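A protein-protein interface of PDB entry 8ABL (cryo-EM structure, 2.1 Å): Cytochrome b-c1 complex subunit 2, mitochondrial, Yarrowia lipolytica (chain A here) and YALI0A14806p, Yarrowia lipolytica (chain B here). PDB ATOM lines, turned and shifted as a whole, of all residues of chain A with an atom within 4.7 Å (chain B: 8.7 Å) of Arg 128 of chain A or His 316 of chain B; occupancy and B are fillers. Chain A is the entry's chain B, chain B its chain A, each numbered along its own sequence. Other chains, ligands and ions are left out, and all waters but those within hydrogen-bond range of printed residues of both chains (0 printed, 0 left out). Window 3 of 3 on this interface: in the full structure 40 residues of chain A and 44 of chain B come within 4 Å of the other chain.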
ATOM      1  N   GLN A  63      14.889 -27.542   4.253  1.00  0.00           N
ATOM      2  CA  GLN A  63      13.660 -27.214   4.968  1.00  0.00           C
ATOM      3  C   GLN A  63      13.705 -27.881   6.336  1.00  0.00           C
ATOM      4  O   GLN A  63      14.785 -28.173   6.828  1.00  0.00           O
ATOM      5  CB  GLN A  63      12.438 -27.634   4.163  1.00  0.00           C
ATOM      6  CG  GLN A  63      12.331 -26.914   2.832  1.00  0.00           C
ATOM      7  CD  GLN A  63      12.201 -25.417   2.975  1.00  0.00           C
ATOM      8  OE1 GLN A  63      11.320 -24.912   3.671  1.00  0.00           O
ATOM      9  NE2 GLN A  63      13.113 -24.697   2.340  1.00  0.00           N
ATOM     10  N   ASN A  64      12.563 -27.994   7.022  1.00  0.00           N
ATOM     11  CA  ASN A  64      12.604 -28.526   8.374  1.00  0.00           C
ATOM     12  C   ASN A  64      13.056 -29.979   8.322  1.00  0.00           C
ATOM     13  O   ASN A  64      12.524 -30.786   7.569  1.00  0.00           O
ATOM     14  CB  ASN A  64      11.256 -28.416   9.084  1.00  0.00           C
ATOM     15  CG  ASN A  64      10.798 -26.988   9.306  1.00  0.00           C
ATOM     16  OD1 ASN A  64      11.605 -26.092   9.539  1.00  0.00           O
ATOM     17  ND2 ASN A  64       9.499 -26.759   9.219  1.00  0.00           N
ATOM     18  N   ALA A  70      14.453 -25.479   9.511  1.00  0.00           N
ATOM     19  CA  ALA A  70      14.979 -24.582   8.493  1.00  0.00           C
ATOM     20  C   ALA A  70      15.494 -23.286   9.133  1.00  0.00           C
ATOM     21  O   ALA A  70      16.593 -22.818   8.824  1.00  0.00           O
ATOM     22  CB  ALA A  70      13.894 -24.342   7.470  1.00  0.00           C
ATOM     23  N   LEU A  71      14.712 -22.747  10.076  1.00  0.00           N
ATOM     24  CA  LEU A  71      15.043 -21.500  10.737  1.00  0.00           C
ATOM     25  C   LEU A  71      16.336 -21.661  11.516  1.00  0.00           C
ATOM     26  O   LEU A  71      17.223 -20.826  11.407  1.00  0.00           O
ATOM     27  CB  LEU A  71      13.893 -21.068  11.648  1.00  0.00           C
ATOM     28  CG  LEU A  71      14.263 -20.077  12.753  1.00  0.00           C
ATOM     29  CD1 LEU A  71      14.583 -18.692  12.185  1.00  0.00           C
ATOM     30  CD2 LEU A  71      13.135 -19.982  13.764  1.00  0.00           C
ATOM     31  N   VAL A  74      19.383 -21.815   9.128  1.00  0.00           N
ATOM     32  CA  VAL A  74      19.794 -20.551   8.539  1.00  0.00           C
ATOM     33  C   VAL A  74      20.468 -19.669   9.585  1.00  0.00           C
ATOM     34  O   VAL A  74      21.433 -18.988   9.267  1.00  0.00           O
ATOM     35  CB  VAL A  74      18.609 -19.823   7.892  1.00  0.00           C
ATOM     36  CG1 VAL A  74      18.942 -18.383   7.520  1.00  0.00           C
ATOM     37  CG2 VAL A  74      18.097 -20.587   6.689  1.00  0.00           C
ATOM     38  N   ARG A  75      19.970 -19.668  10.823  1.00  0.00           N
ATOM     39  CA  ARG A  75      20.573 -18.800  11.824  1.00  0.00           C
ATOM     40  C   ARG A  75      21.986 -19.281  12.138  1.00  0.00           C
ATOM     41  O   ARG A  75      22.855 -18.475  12.437  1.00  0.00           O
ATOM     42  CB  ARG A  75      19.731 -18.686  13.100  1.00  0.00           C
ATOM     43  CG  ARG A  75      18.401 -17.964  12.926  1.00  0.00           C
ATOM     44  CD  ARG A  75      18.449 -16.571  12.319  1.00  0.00           C
ATOM     45  NE  ARG A  75      17.094 -16.029  12.273  1.00  0.00           N
ATOM     46  CZ  ARG A  75      16.502 -15.372  13.267  1.00  0.00           C
ATOM     47  NH1 ARG A  75      17.156 -15.131  14.391  1.00  0.00           N
ATOM     48  NH2 ARG A  75      15.265 -14.936  13.124  1.00  0.00           N
ATOM     49  N   PHE A 123       2.615 -27.529   4.566  1.00  0.00           N
ATOM     50  CA  PHE A 123       2.663 -26.074   4.616  1.00  0.00           C
ATOM     51  C   PHE A 123       3.972 -25.563   4.015  1.00  0.00           C
ATOM     52  O   PHE A 123       3.977 -24.478   3.453  1.00  0.00           O
ATOM     53  CB  PHE A 123       2.415 -25.503   6.017  1.00  0.00           C
ATOM     54  CG  PHE A 123       3.602 -25.603   6.940  1.00  0.00           C
ATOM     55  CD1 PHE A 123       4.619 -24.652   6.902  1.00  0.00           C
ATOM     56  CD2 PHE A 123       3.726 -26.672   7.817  1.00  0.00           C
ATOM     57  CE1 PHE A 123       5.727 -24.766   7.732  1.00  0.00           C
ATOM     58  CE2 PHE A 123       4.825 -26.775   8.661  1.00  0.00           C
ATOM     59  CZ  PHE A 123       5.821 -25.820   8.620  1.00  0.00           C
ATOM     60  N   GLU A 124       5.075 -26.318   4.157  1.00  0.00           N
ATOM     61  CA  GLU A 124       6.338 -25.895   3.565  1.00  0.00           C
ATOM     62  C   GLU A 124       6.194 -25.894   2.050  1.00  0.00           C
ATOM     63  O   GLU A 124       6.670 -24.973   1.390  1.00  0.00           O
ATOM     64  CB  GLU A 124       7.530 -26.776   3.949  1.00  0.00           C
ATOM     65  CG  GLU A 124       7.741 -26.865   5.439  1.00  0.00           C
ATOM     66  CD  GLU A 124       9.074 -27.434   5.901  1.00  0.00           C
ATOM     67  OE1 GLU A 124       9.176 -28.669   5.969  1.00  0.00           O
ATOM     68  OE2 GLU A 124      10.007 -26.636   6.209  1.00  0.00           O
ATOM     69  N   LEU A 125       5.532 -26.924   1.509  1.00  0.00           N
ATOM     70  CA  LEU A 125       5.323 -26.967   0.071  1.00  0.00           C
ATOM     71  C   LEU A 125       4.494 -25.766  -0.384  1.00  0.00           C
ATOM     72  O   LEU A 125       4.873 -25.065  -1.310  1.00  0.00           O
ATOM     73  CB  LEU A 125       4.689 -28.300  -0.337  1.00  0.00           C
ATOM     74  CG  LEU A 125       4.329 -28.442  -1.813  1.00  0.00           C
ATOM     75  CD1 LEU A 125       5.567 -28.331  -2.704  1.00  0.00           C
ATOM     76  CD2 LEU A 125       3.634 -29.772  -2.042  1.00  0.00           C
ATOM     77  N   THR A 126       3.393 -25.476   0.301  1.00  0.00           N
ATOM     78  CA  THR A 126       2.506 -24.424  -0.168  1.00  0.00           C
ATOM     79  C   THR A 126       3.093 -23.027   0.041  1.00  0.00           C
ATOM     80  O   THR A 126       2.919 -22.135  -0.788  1.00  0.00           O
ATOM     81  CB  THR A 126       1.200 -24.520   0.614  1.00  0.00           C
ATOM     82  OG1 THR A 126       0.685 -25.825   0.357  1.00  0.00           O
ATOM     83  CG2 THR A 126       0.206 -23.447   0.235  1.00  0.00           C
ATOM     84  N   GLU A 127       3.746 -22.815   1.179  1.00  0.00           N
ATOM     85  CA  GLU A 127       4.088 -21.457   1.564  1.00  0.00           C
ATOM     86  C   GLU A 127       5.542 -21.127   1.226  1.00  0.00           C
ATOM     87  O   GLU A 127       5.875 -19.960   1.061  1.00  0.00           O
ATOM     88  CB  GLU A 127       3.854 -21.255   3.061  1.00  0.00           C
ATOM     89  CG  GLU A 127       2.398 -21.357   3.523  1.00  0.00           C
ATOM     90  CD  GLU A 127       2.161 -21.576   5.019  1.00  0.00           C
ATOM     91  OE1 GLU A 127       2.989 -21.104   5.834  1.00  0.00           O
ATOM     92  OE2 GLU A 127       1.146 -22.226   5.372  1.00  0.00           O
ATOM     93  N   ARG A 128       6.421 -22.128   1.202  1.00  0.00           N
ATOM     94  CA  ARG A 128       7.844 -21.844   1.122  1.00  0.00           C
ATOM     95  C   ARG A 128       8.400 -22.335  -0.205  1.00  0.00           C
ATOM     96  O   ARG A 128       8.891 -21.539  -0.995  1.00  0.00           O
ATOM     97  CB  ARG A 128       8.559 -22.404   2.348  1.00  0.00           C
ATOM     98  CG  ARG A 128       8.125 -21.664   3.595  1.00  0.00           C
ATOM     99  CD  ARG A 128       8.710 -22.395   4.770  1.00  0.00           C
ATOM    100  NE  ARG A 128       8.185 -21.705   5.933  1.00  0.00           N
ATOM    101  CZ  ARG A 128       8.617 -21.852   7.179  1.00  0.00           C
ATOM    102  NH1 ARG A 128       9.610 -22.681   7.461  1.00  0.00           N
ATOM    103  NH2 ARG A 128       8.052 -21.150   8.144  1.00  0.00           N
ATOM    104  N   VAL A 129       8.221 -23.625  -0.476  1.00  0.00           N
ATOM    105  CA  VAL A 129       8.943 -24.304  -1.532  1.00  0.00           C
ATOM    106  C   VAL A 129       8.336 -23.948  -2.886  1.00  0.00           C
ATOM    107  O   VAL A 129       9.035 -23.453  -3.755  1.00  0.00           O
ATOM    108  CB  VAL A 129       8.986 -25.814  -1.258  1.00  0.00           C
ATOM    109  CG1 VAL A 129       9.516 -26.577  -2.459  1.00  0.00           C
ATOM    110  CG2 VAL A 129       9.823 -26.108  -0.024  1.00  0.00           C
ATOM    111  N   ALA A 130       7.034 -24.157  -3.072  1.00  0.00           N
ATOM    112  CA  ALA A 130       6.467 -23.907  -4.390  1.00  0.00           C
ATOM    113  C   ALA A 130       6.584 -22.434  -4.800  1.00  0.00           C
ATOM    114  O   ALA A 130       6.903 -22.156  -5.950  1.00  0.00           O
ATOM    115  CB  ALA A 130       5.055 -24.417  -4.476  1.00  0.00           C
ATOM    116  N   PRO A 131       6.324 -21.433  -3.925  1.00  0.00           N
ATOM    117  CA  PRO A 131       6.532 -20.031  -4.315  1.00  0.00           C
ATOM    118  C   PRO A 131       7.952 -19.666  -4.761  1.00  0.00           C
ATOM    119  O   PRO A 131       8.134 -18.865  -5.676  1.00  0.00           O
ATOM    120  CB  PRO A 131       6.113 -19.252  -3.061  1.00  0.00           C
ATOM    121  CG  PRO A 131       5.140 -20.188  -2.363  1.00  0.00           C
ATOM    122  CD  PRO A 131       5.725 -21.567  -2.583  1.00  0.00           C
ATOM    123  N   VAL A 132       8.946 -20.261  -4.102  1.00  0.00           N
ATOM    124  CA  VAL A 132      10.332 -20.025  -4.451  1.00  0.00           C
ATOM    125  C   VAL A 132      10.634 -20.690  -5.798  1.00  0.00           C
ATOM    126  O   VAL A 132      11.287 -20.079  -6.638  1.00  0.00           O
ATOM    127  CB  VAL A 132      11.268 -20.480  -3.317  1.00  0.00           C
ATOM    128  CG1 VAL A 132      12.670 -20.781  -3.813  1.00  0.00           C
ATOM    129  CG2 VAL A 132      11.328 -19.444  -2.207  1.00  0.00           C
ATOM    130  N   TYR B 307      18.327  -8.720   1.597  1.00  0.00           N
ATOM    131  CA  TYR B 307      17.160  -9.565   1.648  1.00  0.00           C
ATOM    132  C   TYR B 307      16.683  -9.742   0.225  1.00  0.00           C
ATOM    133  O   TYR B 307      16.725  -8.784  -0.532  1.00  0.00           O
ATOM    134  CB  TYR B 307      16.040  -8.850   2.400  1.00  0.00           C
ATOM    135  CG  TYR B 307      14.696  -9.503   2.228  1.00  0.00           C
ATOM    136  CD1 TYR B 307      14.392 -10.670   2.912  1.00  0.00           C
ATOM    137  CD2 TYR B 307      13.763  -8.992   1.334  1.00  0.00           C
ATOM    138  CE1 TYR B 307      13.169 -11.297   2.745  1.00  0.00           C
ATOM    139  CE2 TYR B 307      12.525  -9.592   1.174  1.00  0.00           C
ATOM    140  CZ  TYR B 307      12.234 -10.747   1.879  1.00  0.00           C
ATOM    141  OH  TYR B 307      11.016 -11.331   1.704  1.00  0.00           O
ATOM    142  N   ASP B 308      16.167 -10.925  -0.108  1.00  0.00           N
ATOM    143  CA  ASP B 308      15.597 -11.141  -1.424  1.00  0.00           C
ATOM    144  C   ASP B 308      14.503 -12.190  -1.301  1.00  0.00           C
ATOM    145  O   ASP B 308      14.804 -13.318  -0.940  1.00  0.00           O
ATOM    146  CB  ASP B 308      16.688 -11.618  -2.385  1.00  0.00           C
ATOM    147  CG  ASP B 308      16.195 -11.886  -3.794  1.00  0.00           C
ATOM    148  OD1 ASP B 308      15.106 -11.382  -4.153  1.00  0.00           O
ATOM    149  OD2 ASP B 308      16.922 -12.571  -4.540  1.00  0.00           O
ATOM    150  N   ARG B 309      13.261 -11.844  -1.662  1.00  0.00           N
ATOM    151  CA  ARG B 309      12.151 -12.769  -1.470  1.00  0.00           C
ATOM    152  C   ARG B 309      12.330 -14.030  -2.319  1.00  0.00           C
ATOM    153  O   ARG B 309      11.783 -15.066  -1.987  1.00  0.00           O
ATOM    154  CB  ARG B 309      10.774 -12.115  -1.668  1.00  0.00           C
ATOM    155  CG  ARG B 309      10.436 -11.813  -3.121  1.00  0.00           C
ATOM    156  CD  ARG B 309       9.007 -11.441  -3.460  1.00  0.00           C
ATOM    157  NE  ARG B 309       9.022 -11.125  -4.890  1.00  0.00           N
ATOM    158  CZ  ARG B 309       8.000 -10.681  -5.631  1.00  0.00           C
ATOM    159  NH1 ARG B 309       6.812 -10.447  -5.096  1.00  0.00           N
ATOM    160  NH2 ARG B 309       8.187 -10.439  -6.918  1.00  0.00           N
ATOM    161  N   ALA B 310      13.147 -13.972  -3.369  1.00  0.00           N
ATOM    162  CA  ALA B 310      13.320 -15.117  -4.249  1.00  0.00           C
ATOM    163  C   ALA B 310      14.280 -16.153  -3.664  1.00  0.00           C
ATOM    164  O   ALA B 310      14.367 -17.272  -4.158  1.00  0.00           O
ATOM    165  CB  ALA B 310      13.814 -14.623  -5.576  1.00  0.00           C
ATOM    166  N   VAL B 311      15.065 -15.774  -2.672  1.00  0.00           N
ATOM    167  CA  VAL B 311      15.966 -16.749  -2.095  1.00  0.00           C
ATOM    168  C   VAL B 311      15.222 -17.412  -0.946  1.00  0.00           C
ATOM    169  O   VAL B 311      14.604 -16.710  -0.156  1.00  0.00           O
ATOM    170  CB  VAL B 311      17.202 -15.991  -1.609  1.00  0.00           C
ATOM    171  CG1 VAL B 311      18.107 -16.843  -0.746  1.00  0.00           C
ATOM    172  CG2 VAL B 311      17.950 -15.352  -2.766  1.00  0.00           C
ATOM    173  N   GLY B 312      15.293 -18.744  -0.852  1.00  0.00           N
ATOM    174  CA  GLY B 312      14.535 -19.506   0.129  1.00  0.00           C
ATOM    175  C   GLY B 312      14.930 -19.192   1.573  1.00  0.00           C
ATOM    176  O   GLY B 312      14.070 -19.099   2.448  1.00  0.00           O
ATOM    177  N   THR B 313      16.231 -19.004   1.814  1.00  0.00           N
ATOM    178  CA  THR B 313      16.720 -18.777   3.163  1.00  0.00           C
ATOM    179  C   THR B 313      16.385 -17.379   3.695  1.00  0.00           C
ATOM    180  O   THR B 313      16.525 -17.167   4.896  1.00  0.00           O
ATOM    181  CB  THR B 313      18.236 -18.983   3.254  1.00  0.00           C
ATOM    182  OG1 THR B 313      18.783 -18.091   2.287  1.00  0.00           O
ATOM    183  CG2 THR B 313      18.673 -20.405   2.976  1.00  0.00           C
ATOM    184  N   SER B 314      15.978 -16.421   2.844  1.00  0.00           N
ATOM    185  CA  SER B 314      15.929 -15.028   3.288  1.00  0.00           C
ATOM    186  C   SER B 314      14.856 -14.780   4.348  1.00  0.00           C
ATOM    187  O   SER B 314      14.996 -13.891   5.179  1.00  0.00           O
ATOM    188  CB  SER B 314      15.763 -14.074   2.148  1.00  0.00           C
ATOM    189  OG  SER B 314      14.497 -14.299   1.559  1.00  0.00           O
ATOM    190  N   ARG B 315      13.791 -15.573   4.342  1.00  0.00           N
ATOM    191  CA  ARG B 315      12.772 -15.399   5.360  1.00  0.00           C
ATOM    192  C   ARG B 315      13.286 -15.806   6.742  1.00  0.00           C
ATOM    193  O   ARG B 315      12.655 -15.474   7.730  1.00  0.00           O
ATOM    194  CB  ARG B 315      11.519 -16.181   4.985  1.00  0.00           C
ATOM    195  CG  ARG B 315      11.632 -17.661   5.301  1.00  0.00           C
ATOM    196  CD  ARG B 315      10.297 -18.369   5.187  1.00  0.00           C
ATOM    197  NE  ARG B 315       9.865 -18.431   3.793  1.00  0.00           N
ATOM    198  CZ  ARG B 315       8.794 -17.827   3.281  1.00  0.00           C
ATOM    199  NH1 ARG B 315       7.978 -17.118   4.046  1.00  0.00           N
ATOM    200  NH2 ARG B 315       8.523 -17.962   1.994  1.00  0.00           N
ATOM    201  N   HIS B 316      14.428 -16.490   6.832  1.00  0.00           N
ATOM    202  CA  HIS B 316      14.873 -16.935   8.143  1.00  0.00           C
ATOM    203  C   HIS B 316      16.075 -16.158   8.670  1.00  0.00           C
ATOM    204  O   HIS B 316      16.670 -16.574   9.661  1.00  0.00           O
ATOM    205  CB  HIS B 316      15.206 -18.419   8.095  1.00  0.00           C
ATOM    206  CG  HIS B 316      14.031 -19.276   7.776  1.00  0.00           C
ATOM    207  ND1 HIS B 316      12.834 -19.188   8.465  1.00  0.00           N
ATOM    208  CD2 HIS B 316      13.861 -20.237   6.846  1.00  0.00           C
ATOM    209  CE1 HIS B 316      11.982 -20.073   7.981  1.00  0.00           C
ATOM    210  NE2 HIS B 316      12.589 -20.729   6.985  1.00  0.00           N
ATOM    211  N   GLN B 317      16.435 -15.044   8.033  1.00  0.00           N
ATOM    212  CA  GLN B 317      17.661 -14.338   8.378  1.00  0.00           C
ATOM    213  C   GLN B 317      17.506 -13.677   9.744  1.00  0.00           C
ATOM    214  O   GLN B 317      16.400 -13.337  10.155  1.00  0.00           O
ATOM    215  CB  GLN B 317      17.978 -13.278   7.326  1.00  0.00           C
ATOM    216  CG  GLN B 317      18.403 -13.847   5.983  1.00  0.00           C
ATOM    217  CD  GLN B 317      18.783 -12.779   4.982  1.00  0.00           C
ATOM    218  OE1 GLN B 317      19.872 -12.801   4.417  1.00  0.00           O
ATOM    219  NE2 GLN B 317      17.890 -11.833   4.742  1.00  0.00           N
ATOM    220  N   GLY B 318      18.638 -13.473  10.424  1.00  0.00           N
ATOM    221  CA  GLY B 318      18.689 -12.901  11.765  1.00  0.00           C
ATOM    222  C   GLY B 318      18.383 -11.401  11.837  1.00  0.00           C
ATOM    223  O   GLY B 318      17.871 -10.923  12.855  1.00  0.00           O
ATOM    224  N   SER B 319      18.712 -10.668  10.766  1.00  0.00           N
ATOM    225  CA  SER B 319      18.515  -9.230  10.648  1.00  0.00           C
ATOM    226  C   SER B 319      17.085  -8.850  11.002  1.00  0.00           C
ATOM    227  O   SER B 319      16.136  -9.378  10.432  1.00  0.00           O
ATOM    228  CB  SER B 319      18.852  -8.791   9.243  1.00  0.00           C
ATOM    229  OG  SER B 319      18.379  -7.479   8.934  1.00  0.00           O
ATOM    230  N   SER B 322      15.161  -7.553   7.970  1.00  0.00           N
ATOM    231  CA  SER B 322      14.773  -8.658   7.111  1.00  0.00           C
ATOM    232  C   SER B 322      13.475  -9.279   7.635  1.00  0.00           C
ATOM    233  O   SER B 322      12.565  -9.563   6.865  1.00  0.00           O
ATOM    234  CB  SER B 322      15.887  -9.665   7.049  1.00  0.00           C
ATOM    235  OG  SER B 322      15.538 -10.743   6.206  1.00  0.00           O
ATOM    236  N   ASN B 323      13.380  -9.477   8.950  1.00  0.00           N
ATOM    237  CA  ASN B 323      12.179 -10.056   9.533  1.00  0.00           C
ATOM    238  C   ASN B 323      10.965  -9.153   9.330  1.00  0.00           C
ATOM    239  O   ASN B 323       9.916  -9.628   8.908  1.00  0.00           O
ATOM    240  CB  ASN B 323      12.408 -10.358  11.007  1.00  0.00           C
ATOM    241  CG  ASN B 323      13.263 -11.592  11.180  1.00  0.00           C
ATOM    242  OD1 ASN B 323      12.762 -12.697  10.997  1.00  0.00           O
ATOM    243  ND2 ASN B 323      14.536 -11.430  11.521  1.00  0.00           N
ATOM    244  N   SER B 326      10.062  -9.240   5.455  1.00  0.00           N
ATOM    245  CA  SER B 326       9.482 -10.482   4.964  1.00  0.00           C
ATOM    246  C   SER B 326       8.109 -10.736   5.582  1.00  0.00           C
ATOM    247  O   SER B 326       7.188 -11.058   4.849  1.00  0.00           O
ATOM    248  CB  SER B 326      10.392 -11.661   5.112  1.00  0.00           C
ATOM    249  OG  SER B 326      10.760 -11.819   6.462  1.00  0.00           O
ATOM    250  N   ARG B 384      27.542 -11.294  15.975  1.00  0.00           N
ATOM    251  CA  ARG B 384      26.932 -12.037  14.889  1.00  0.00           C
ATOM    252  C   ARG B 384      27.424 -11.535  13.531  1.00  0.00           C
ATOM    253  O   ARG B 384      27.730 -12.345  12.664  1.00  0.00           O
ATOM    254  CB  ARG B 384      25.409 -11.971  14.979  1.00  0.00           C
ATOM    255  CG  ARG B 384      24.806 -12.944  15.981  1.00  0.00           C
ATOM    256  CD  ARG B 384      23.295 -13.099  15.840  1.00  0.00           C
ATOM    257  NE  ARG B 384      22.582 -11.866  16.177  1.00  0.00           N
ATOM    258  CZ  ARG B 384      21.760 -11.194  15.362  1.00  0.00           C
ATOM    259  NH1 ARG B 384      21.190 -10.079  15.787  1.00  0.00           N
ATOM    260  NH2 ARG B 384      21.510 -11.629  14.136  1.00  0.00           N
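Among the printed residues, pairs that only touch across the chains: Arg 75 of chain A with Gly 318 of chain B, Arg 128 of chain A with His 316 of chain B, Val 74 of chain A with His 316 of chain B, Arg 128 of chain A with Arg 315 of chain B, Val 74 of chain A with Thr 313 of chain B, Leu 71 of chain A with His 316 of chain B, Ala 70 of chain A with His 316 of chain B, Val 132 of chain A with Ala 310 of chain B, Arg 75 of chain A with Asn 323 of chain B and Val 132 of chain A with Gly 312 of chain B.
Of the 17 printed residues of chain B, 8 touch a printed residue of chain A. Hydrophobic or aromatic side chains of chain B within 4 Å of the printed part of chain A: His 316. Hydrophobic or aromatic side chains of chain A within 4 Å of the printed part of chain B: Ala 70, Leu 71, Val 74 and Val 132. Along chain A the printed residues that touch a printed residue of chain B span positions 70 to 132. Among the printed residues, 13 pairs touch across the chains. Among the printed residues, no Asp or Glu carboxylate lies within 4 Å of a Lys or Arg side-chain nitrogen of the other chain.
Arg 128 of chain A touches two residues of chain B. Of the printed residues of chain A, His 316 of chain B touches Ala 70 (3.9 Å), Leu 71 (3.8 Å), Val 74 (3.6 Å), Arg 75 (2.7 Å) and Arg 128 (3.6 Å). Of the printed residues of chain B, Glu 127 of chain A touches Arg 315 (3.4 Å). Of the printed residues of chain A, Arg 315 of chain B touches Glu 127 and Arg 128. Printed residues of chain B within 4 Å of Leu 71 of chain A: His 316 (3.8 Å). Gln 63 of chain A touches none of the printed residues of chain B. The nearest printed residue of chain A that does not touch His 316 of chain B is Gln 63 of chain A (5.5 Å).
The side-chain carboxylate (OD1) of Asp 308 of chain B lies close to the backbone NH (N) of Ala 310 of chain B, at 3.3 Å. The side-chain hydroxyl of Ser 322 of chain B is in hydrogen-bond range of the side-chain amide nitrogen of Gln 317 of chain B (3.0 Å). The backbone carbonyl oxygen (O) of Gln 317 of chain B sits at hydrogen-bond distance from the side-chain amide nitrogen (ND2) of Asn 323 of chain B (3.0 Å). O of Ser 319 of chain B lies within hydrogen-bond range of ND2 of Asn 323 of chain B, at 2.8 Å. O of Asn 323 of chain B sits at hydrogen-bond distance from OG of Ser 326 of chain B, at 3.4 Å. The backbone NH (N) of Ala 70 of chain A sits at hydrogen-bond distance from the side-chain amide oxygen (OD1) of Asn 64 of chain A (2.9 Å).
NH2 of Arg 315 of chain B is in hydrogen-bond range of O of Glu 127 of chain A, 3.4 Å away. O of His 316 of chain B lies within hydrogen-bond range of NE of Arg 75 of chain A, at 2.7 Å. O of Gln 317 of chain B sits close to NE of Arg 75 of chain A (3.5 Å).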
